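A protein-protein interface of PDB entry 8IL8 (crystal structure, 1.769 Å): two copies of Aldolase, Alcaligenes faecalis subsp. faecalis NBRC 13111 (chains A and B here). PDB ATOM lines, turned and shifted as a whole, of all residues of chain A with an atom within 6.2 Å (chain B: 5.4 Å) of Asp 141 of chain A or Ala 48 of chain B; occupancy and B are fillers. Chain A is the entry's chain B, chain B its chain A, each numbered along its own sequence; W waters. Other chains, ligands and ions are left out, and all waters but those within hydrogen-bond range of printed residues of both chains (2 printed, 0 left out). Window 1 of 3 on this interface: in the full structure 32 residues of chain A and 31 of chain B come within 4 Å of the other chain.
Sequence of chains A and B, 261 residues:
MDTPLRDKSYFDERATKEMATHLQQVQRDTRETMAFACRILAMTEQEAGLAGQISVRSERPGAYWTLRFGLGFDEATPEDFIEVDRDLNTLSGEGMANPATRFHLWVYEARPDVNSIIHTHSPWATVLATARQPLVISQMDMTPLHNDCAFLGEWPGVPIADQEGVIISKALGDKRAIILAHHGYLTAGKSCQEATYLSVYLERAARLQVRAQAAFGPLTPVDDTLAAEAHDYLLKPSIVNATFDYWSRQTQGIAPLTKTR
Of the 9 printed residues of chain B, 5 touch a printed residue of chain A.
Hydrophobic or aromatic side chains of chain B that line the printed part of chain A: Ala 48 and His 121.
Hydrophobic or aromatic side chains of chain A within 4 Å of the printed part of chain B: Tyr 201 and Trp 247.
Along chain A the printed residues that touch a printed residue of chain B span positions 139 to 247.
Among the printed residues, 10 pairs touch across the chains.
Among the printed residues, Asp or Glu carboxylates within 4 Å of a Lys or Arg side-chain nitrogen of the other chain: Arg 204 of chain A with Glu 47 of chain B.
N of Gln 139 of chain A is in hydrogen-bond range of SD of Met 142 of chain A, 3.7 Å away.
The side-chain carboxylate of Glu 47 of chain B lies within hydrogen-bond range of the backbone NH of Gly 49 of chain B, 2.9 Å away.
N of Asp 141 of chain A lies within hydrogen-bond range of OE1 of Gln 139 of chain A (2.9 Å).
Water W1 lies within hydrogen-bond range of the side-chain carboxylate (OD1) of Asp 141 of chain A (2.7 Å), the backbone carbonyl oxygen (O) of Ala 48 of chain B (2.7 Å) and the side-chain hydroxyl (OH) of Tyr 201 of chain A (2.9 Å).
Water W2 bridges OH of Tyr 201 of chain A and N of Leu 50 of chain B.
OE2 of Glu 47 of chain B sits at hydrogen-bond distance from NE1 of Trp 247 of chain A.
The side-chain amide nitrogen (NE2) of Gln 139 of chain A is in hydrogen-bond range of the backbone carbonyl oxygen (O) of His 183 of chain B (2.9 Å).
ND1 of His 121 of chain B is in hydrogen-bond range of OD2 of Asp 141 of chain A.
The side-chain carboxylate (OE2) of Glu 47 of chain B is in salt-bridge range of the guanidinium group (NH2) of Arg 204 of chain A.
No position is printed for both chains.
Printed residues of chain B within 4 Å of Gln 139 of chain A: His 121 and His 183.
Asp 141 of chain A touches just these residues of chain B: Ala 48 and His 121.
Pro 144 of chain A touches none of the printed residues of chain B.
Leu 234 of chain A touches none of the printed residues of chain B.
Printed residues of chain B within 4 Å of Trp 247 of chain A: Glu 47 (3.0 Å).
Of the printed residues of chain A, Glu 47 of chain B touches Arg 204 and Trp 247.
The nearest printed residue of chain B that does not touch Asp 141 of chain A is His 183 of chain B (4.9 Å).
The nearest residue of chain A that does not touch Ala 48 of chain B is Trp 247 of chain A (5.8 Å).
Among the printed residues, pairs that only touch across the chains: Arg 204 of chain A with Gly 49 of chain B, Tyr 201 of chain A with Gly 49 of chain B, Tyr 201 of chain A with Ala 48 of chain B, Arg 204 of chain A with Ala 48 of chain B, Asp 141 of chain A with Ala 48 of chain B and Gln 139 of chain A with His 121 of chain B.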
ATOM      1  N   GLN A 139     -19.778 -11.235 -13.851  1.00  0.00           N
ATOM      2  CA  GLN A 139     -18.429 -11.732 -14.102  1.00  0.00           C
ATOM      3  C   GLN A 139     -17.849 -11.052 -15.339  1.00  0.00           C
ATOM      4  O   GLN A 139     -18.599 -10.631 -16.220  1.00  0.00           O
ATOM      5  CB  GLN A 139     -18.456 -13.277 -14.235  1.00  0.00           C
ATOM      6  CG  GLN A 139     -17.069 -13.960 -14.286  1.00  0.00           C
ATOM      7  CD  GLN A 139     -16.599 -14.173 -15.714  1.00  0.00           C
ATOM      8  OE1 GLN A 139     -17.381 -14.086 -16.675  1.00  0.00           O
ATOM      9  NE2 GLN A 139     -15.314 -14.375 -15.915  1.00  0.00           N
ATOM     10  N   MET A 140     -16.519 -10.873 -15.353  1.00  0.00           N
ATOM     11  CA  MET A 140     -15.742 -10.236 -16.424  1.00  0.00           C
ATOM     12  C   MET A 140     -16.224 -10.561 -17.865  1.00  0.00           C
ATOM     13  O   MET A 140     -16.432  -9.649 -18.647  1.00  0.00           O
ATOM     14  CB  MET A 140     -14.246 -10.585 -16.245  1.00  0.00           C
ATOM     15  CG  MET A 140     -13.375 -10.013 -17.308  1.00  0.00           C
ATOM     16  SD  MET A 140     -13.343  -8.182 -17.322  1.00  0.00           S
ATOM     17  CE  MET A 140     -12.327  -7.935 -18.729  1.00  0.00           C
ATOM     18  N   ASP A 141     -16.361 -11.851 -18.212  1.00  0.00           N
ATOM     19  CA  ASP A 141     -16.771 -12.310 -19.545  1.00  0.00           C
ATOM     20  C   ASP A 141     -18.254 -12.121 -19.856  1.00  0.00           C
ATOM     21  O   ASP A 141     -18.657 -12.374 -20.983  1.00  0.00           O
ATOM     22  CB  ASP A 141     -16.354 -13.776 -19.764  1.00  0.00           C
ATOM     23  CG  ASP A 141     -14.866 -13.933 -19.551  1.00  0.00           C
ATOM     24  OD1 ASP A 141     -14.116 -13.033 -19.981  1.00  0.00           O
ATOM     25  OD2 ASP A 141     -14.454 -14.940 -18.912  1.00  0.00           O
ATOM     26  N   MET A 142     -19.074 -11.777 -18.855  1.00  0.00           N
ATOM     27  CA  MET A 142     -20.479 -11.457 -19.063  1.00  0.00           C
ATOM     28  C   MET A 142     -20.646  -9.988 -19.483  1.00  0.00           C
ATOM     29  O   MET A 142     -21.711  -9.642 -19.997  1.00  0.00           O
ATOM     30  CB  MET A 142     -21.284 -11.681 -17.780  1.00  0.00           C
ATOM     31  CG  MET A 142     -21.101 -13.080 -17.191  1.00  0.00           C
ATOM     32  SD  MET A 142     -22.182 -13.310 -15.776  1.00  0.00           S
ATOM     33  CE  MET A 142     -23.684 -13.743 -16.630  1.00  0.00           C
ATOM     34  N   THR A 143     -19.613  -9.119 -19.251  1.00  0.00           N
ATOM     35  CA  THR A 143     -19.690  -7.680 -19.524  1.00  0.00           C
ATOM     36  C   THR A 143     -19.895  -7.300 -20.999  1.00  0.00           C
ATOM     37  O   THR A 143     -20.535  -6.263 -21.182  1.00  0.00           O
ATOM     38  CB  THR A 143     -18.516  -6.925 -18.898  1.00  0.00           C
ATOM     39  OG1 THR A 143     -17.298  -7.278 -19.547  1.00  0.00           O
ATOM     40  CG2 THR A 143     -18.434  -7.166 -17.397  1.00  0.00           C
ATOM     41  N   PRO A 144     -19.476  -8.037 -22.072  1.00  0.00           N
ATOM     42  CA  PRO A 144     -19.874  -7.610 -23.437  1.00  0.00           C
ATOM     43  C   PRO A 144     -21.404  -7.498 -23.601  1.00  0.00           C
ATOM     44  O   PRO A 144     -21.881  -6.790 -24.484  1.00  0.00           O
ATOM     45  CB  PRO A 144     -19.288  -8.712 -24.326  1.00  0.00           C
ATOM     46  CG  PRO A 144     -18.127  -9.237 -23.541  1.00  0.00           C
ATOM     47  CD  PRO A 144     -18.656  -9.263 -22.138  1.00  0.00           C
ATOM     48  N   LEU A 145     -22.183  -8.147 -22.711  1.00  0.00           N
ATOM     49  CA  LEU A 145     -23.638  -8.073 -22.717  1.00  0.00           C
ATOM     50  C   LEU A 145     -24.208  -7.066 -21.700  1.00  0.00           C
ATOM     51  O   LEU A 145     -25.427  -6.926 -21.649  1.00  0.00           O
ATOM     52  CB  LEU A 145     -24.262  -9.456 -22.410  1.00  0.00           C
ATOM     53  CG  LEU A 145     -24.090 -10.611 -23.389  1.00  0.00           C
ATOM     54  CD1 LEU A 145     -24.330 -10.181 -24.841  1.00  0.00           C
ATOM     55  CD2 LEU A 145     -22.792 -11.381 -23.130  1.00  0.00           C
ATOM     56  N   TYR A 201     -19.917 -15.584 -26.213  1.00  0.00           N
ATOM     57  CA  TYR A 201     -19.880 -14.994 -24.865  1.00  0.00           C
ATOM     58  C   TYR A 201     -21.264 -15.030 -24.164  1.00  0.00           C
ATOM     59  O   TYR A 201     -21.311 -15.296 -22.965  1.00  0.00           O
ATOM     60  CB  TYR A 201     -19.276 -13.565 -24.888  1.00  0.00           C
ATOM     61  CG  TYR A 201     -17.762 -13.567 -24.850  1.00  0.00           C
ATOM     62  CD1 TYR A 201     -17.018 -13.933 -25.965  1.00  0.00           C
ATOM     63  CD2 TYR A 201     -17.076 -13.245 -23.688  1.00  0.00           C
ATOM     64  CE1 TYR A 201     -15.631 -14.000 -25.918  1.00  0.00           C
ATOM     65  CE2 TYR A 201     -15.688 -13.246 -23.645  1.00  0.00           C
ATOM     66  CZ  TYR A 201     -14.966 -13.648 -24.758  1.00  0.00           C
ATOM     67  OH  TYR A 201     -13.582 -13.710 -24.712  1.00  0.00           O
ATOM     68  N   LEU A 202     -22.378 -14.830 -24.899  1.00  0.00           N
ATOM     69  CA  LEU A 202     -23.708 -14.913 -24.293  1.00  0.00           C
ATOM     70  C   LEU A 202     -23.979 -16.335 -23.816  1.00  0.00           C
ATOM     71  O   LEU A 202     -24.445 -16.523 -22.688  1.00  0.00           O
ATOM     72  CB  LEU A 202     -24.831 -14.448 -25.279  1.00  0.00           C
ATOM     73  CG  LEU A 202     -26.264 -14.339 -24.728  1.00  0.00           C
ATOM     74  CD1 LEU A 202     -27.078 -13.389 -25.594  1.00  0.00           C
ATOM     75  CD2 LEU A 202     -26.995 -15.577 -24.854  1.00  0.00           C
ATOM     76  N   ARG A 204     -21.860 -18.658 -22.969  1.00  0.00           N
ATOM     77  CA  ARG A 204     -20.984 -18.976 -21.847  1.00  0.00           C
ATOM     78  C   ARG A 204     -21.409 -18.249 -20.579  1.00  0.00           C
ATOM     79  O   ARG A 204     -21.297 -18.815 -19.498  1.00  0.00           O
ATOM     80  CB  ARG A 204     -19.534 -18.745 -22.235  1.00  0.00           C
ATOM     81  CG  ARG A 204     -19.067 -19.800 -23.235  1.00  0.00           C
ATOM     82  CD  ARG A 204     -17.656 -19.538 -23.687  1.00  0.00           C
ATOM     83  NE  ARG A 204     -17.184 -20.496 -24.690  1.00  0.00           N
ATOM     84  CZ  ARG A 204     -15.964 -20.462 -25.229  1.00  0.00           C
ATOM     85  NH1 ARG A 204     -15.605 -21.367 -26.128  1.00  0.00           N
ATOM     86  NH2 ARG A 204     -15.088 -19.532 -24.855  1.00  0.00           N
ATOM     87  N   ALA A 205     -21.940 -17.023 -20.713  1.00  0.00           N
ATOM     88  CA  ALA A 205     -22.451 -16.202 -19.596  1.00  0.00           C
ATOM     89  C   ALA A 205     -23.723 -16.875 -19.032  1.00  0.00           C
ATOM     90  O   ALA A 205     -23.868 -17.016 -17.821  1.00  0.00           O
ATOM     91  CB  ALA A 205     -22.776 -14.779 -20.079  1.00  0.00           C
ATOM     92  N   LEU A 234     -13.599  -5.435 -23.703  1.00  0.00           N
ATOM     93  CA  LEU A 234     -13.779  -6.705 -24.377  1.00  0.00           C
ATOM     94  C   LEU A 234     -14.403  -6.559 -25.773  1.00  0.00           C
ATOM     95  O   LEU A 234     -14.240  -7.459 -26.589  1.00  0.00           O
ATOM     96  CB  LEU A 234     -14.621  -7.660 -23.525  1.00  0.00           C
ATOM     97  CG  LEU A 234     -13.906  -8.301 -22.312  1.00  0.00           C
ATOM     98  CD1 LEU A 234     -14.802  -9.301 -21.656  1.00  0.00           C
ATOM     99  CD2 LEU A 234     -12.569  -8.964 -22.707  1.00  0.00           C
ATOM    100  N   TRP A 247     -10.534 -18.841 -32.527  1.00  0.00           N
ATOM    101  CA  TRP A 247     -11.587 -19.857 -32.605  1.00  0.00           C
ATOM    102  C   TRP A 247     -11.603 -20.500 -33.999  1.00  0.00           C
ATOM    103  O   TRP A 247     -11.797 -21.692 -34.107  1.00  0.00           O
ATOM    104  CB  TRP A 247     -12.953 -19.208 -32.315  1.00  0.00           C
ATOM    105  CG  TRP A 247     -13.156 -18.756 -30.895  1.00  0.00           C
ATOM    106  CD1 TRP A 247     -12.602 -19.291 -29.773  1.00  0.00           C
ATOM    107  CD2 TRP A 247     -14.057 -17.733 -30.450  1.00  0.00           C
ATOM    108  NE1 TRP A 247     -13.097 -18.661 -28.655  1.00  0.00           N
ATOM    109  CE2 TRP A 247     -13.992 -17.701 -29.040  1.00  0.00           C
ATOM    110  CE3 TRP A 247     -14.914 -16.843 -31.106  1.00  0.00           C
ATOM    111  CZ2 TRP A 247     -14.754 -16.812 -28.275  1.00  0.00           C
ATOM    112  CZ3 TRP A 247     -15.643 -15.936 -30.352  1.00  0.00           C
ATOM    113  CH2 TRP A 247     -15.550 -15.916 -28.957  1.00  0.00           C
ATOM    114  N   GLN B  46     -10.262 -25.363 -19.884  1.00  0.00           N
ATOM    115  CA  GLN B  46     -10.164 -24.026 -19.265  1.00  0.00           C
ATOM    116  C   GLN B  46     -10.280 -22.790 -20.198  1.00  0.00           C
ATOM    117  O   GLN B  46      -9.934 -21.682 -19.767  1.00  0.00           O
ATOM    118  CB  GLN B  46      -8.832 -23.922 -18.477  1.00  0.00           C
ATOM    119  CG  GLN B  46      -8.538 -25.137 -17.595  1.00  0.00           C
ATOM    120  CD  GLN B  46      -7.921 -24.787 -16.250  1.00  0.00           C
ATOM    121  OE1 GLN B  46      -7.560 -23.665 -15.973  1.00  0.00           O
ATOM    122  NE2 GLN B  46      -7.847 -25.732 -15.361  1.00  0.00           N
ATOM    123  N   GLU B  47     -10.763 -22.931 -21.435  1.00  0.00           N
ATOM    124  CA  GLU B  47     -10.846 -21.783 -22.362  1.00  0.00           C
ATOM    125  C   GLU B  47     -11.967 -20.755 -22.057  1.00  0.00           C
ATOM    126  O   GLU B  47     -13.067 -21.122 -21.650  1.00  0.00           O
ATOM    127  CB  GLU B  47     -10.976 -22.296 -23.819  1.00  0.00           C
ATOM    128  CG  GLU B  47     -10.840 -21.240 -24.904  1.00  0.00           C
ATOM    129  CD  GLU B  47     -12.060 -21.104 -25.800  1.00  0.00           C
ATOM    130  OE1 GLU B  47     -12.523 -22.137 -26.334  1.00  0.00           O
ATOM    131  OE2 GLU B  47     -12.563 -19.969 -25.963  1.00  0.00           O
ATOM    132  N   ALA B  48     -11.680 -19.461 -22.293  1.00  0.00           N
ATOM    133  CA  ALA B  48     -12.627 -18.348 -22.189  1.00  0.00           C
ATOM    134  C   ALA B  48     -12.072 -17.265 -23.117  1.00  0.00           C
ATOM    135  O   ALA B  48     -11.637 -16.195 -22.668  1.00  0.00           O
ATOM    136  CB  ALA B  48     -12.731 -17.843 -20.758  1.00  0.00           C
ATOM    137  N   GLY B  49     -12.037 -17.583 -24.411  1.00  0.00           N
ATOM    138  CA  GLY B  49     -11.454 -16.672 -25.392  1.00  0.00           C
ATOM    139  C   GLY B  49      -9.950 -16.584 -25.189  1.00  0.00           C
ATOM    140  O   GLY B  49      -9.305 -17.584 -24.850  1.00  0.00           O
ATOM    141  N   LEU B  50      -9.387 -15.401 -25.347  1.00  0.00           N
ATOM    142  CA  LEU B  50      -7.946 -15.204 -25.171  1.00  0.00           C
ATOM    143  C   LEU B  50      -7.607 -14.716 -23.736  1.00  0.00           C
ATOM    144  O   LEU B  50      -6.625 -13.997 -23.530  1.00  0.00           O
ATOM    145  CB  LEU B  50      -7.442 -14.226 -26.248  1.00  0.00           C
ATOM    146  CG  LEU B  50      -7.455 -14.757 -27.674  1.00  0.00           C
ATOM    147  CD1 LEU B  50      -7.234 -13.622 -28.682  1.00  0.00           C
ATOM    148  CD2 LEU B  50      -6.477 -15.911 -27.841  1.00  0.00           C
ATOM    149  N   ALA B  51      -8.404 -15.125 -22.746  1.00  0.00           N
ATOM    150  CA  ALA B  51      -8.184 -14.697 -21.371  1.00  0.00           C
ATOM    151  C   ALA B  51      -7.077 -15.487 -20.621  1.00  0.00           C
ATOM    152  O   ALA B  51      -6.649 -15.055 -19.551  1.00  0.00           O
ATOM    153  CB  ALA B  51      -9.490 -14.756 -20.592  1.00  0.00           C
ATOM    154  N   GLY B  52      -6.646 -16.613 -21.182  1.00  0.00           N
ATOM    155  CA  GLY B  52      -5.668 -17.502 -20.568  1.00  0.00           C
ATOM    156  C   GLY B  52      -4.268 -16.958 -20.623  1.00  0.00           C
ATOM    157  O   GLY B  52      -3.840 -16.414 -21.645  1.00  0.00           O
ATOM    158  N   HIS B 121     -10.091 -18.077 -16.808  1.00  0.00           N
ATOM    159  CA  HIS B 121     -11.444 -17.909 -16.328  1.00  0.00           C
ATOM    160  C   HIS B 121     -12.106 -19.272 -16.633  1.00  0.00           C
ATOM    161  O   HIS B 121     -13.063 -19.342 -17.381  1.00  0.00           O
ATOM    162  CB  HIS B 121     -12.186 -16.790 -17.074  1.00  0.00           C
ATOM    163  CG  HIS B 121     -11.518 -15.447 -17.117  1.00  0.00           C
ATOM    164  ND1 HIS B 121     -11.972 -14.465 -17.986  1.00  0.00           N
ATOM    165  CD2 HIS B 121     -10.488 -14.946 -16.390  1.00  0.00           C
ATOM    166  CE1 HIS B 121     -11.193 -13.419 -17.785  1.00  0.00           C
ATOM    167  NE2 HIS B 121     -10.288 -13.652 -16.832  1.00  0.00           N
ATOM    168  N   HIS B 183     -14.331 -12.888 -11.693  1.00  0.00           N
ATOM    169  CA  HIS B 183     -13.260 -12.885 -12.677  1.00  0.00           C
ATOM    170  C   HIS B 183     -12.787 -14.305 -13.056  1.00  0.00           C
ATOM    171  O   HIS B 183     -13.086 -14.748 -14.160  1.00  0.00           O
ATOM    172  CB  HIS B 183     -12.125 -11.988 -12.133  1.00  0.00           C
ATOM    173  CG  HIS B 183     -10.950 -11.815 -13.044  1.00  0.00           C
ATOM    174  ND1 HIS B 183      -9.828 -11.150 -12.625  1.00  0.00           N
ATOM    175  CD2 HIS B 183     -10.773 -12.204 -14.328  1.00  0.00           C
ATOM    176  CE1 HIS B 183      -8.987 -11.179 -13.638  1.00  0.00           C
ATOM    177  NE2 HIS B 183      -9.499 -11.824 -14.677  1.00  0.00           N
HETATM  178  O   HOH W   1     -12.536 -13.675 -22.047  1.00  0.00           O
HETATM  179  O   HOH W   2     -11.038 -12.884 -25.907  1.00  0.00           O
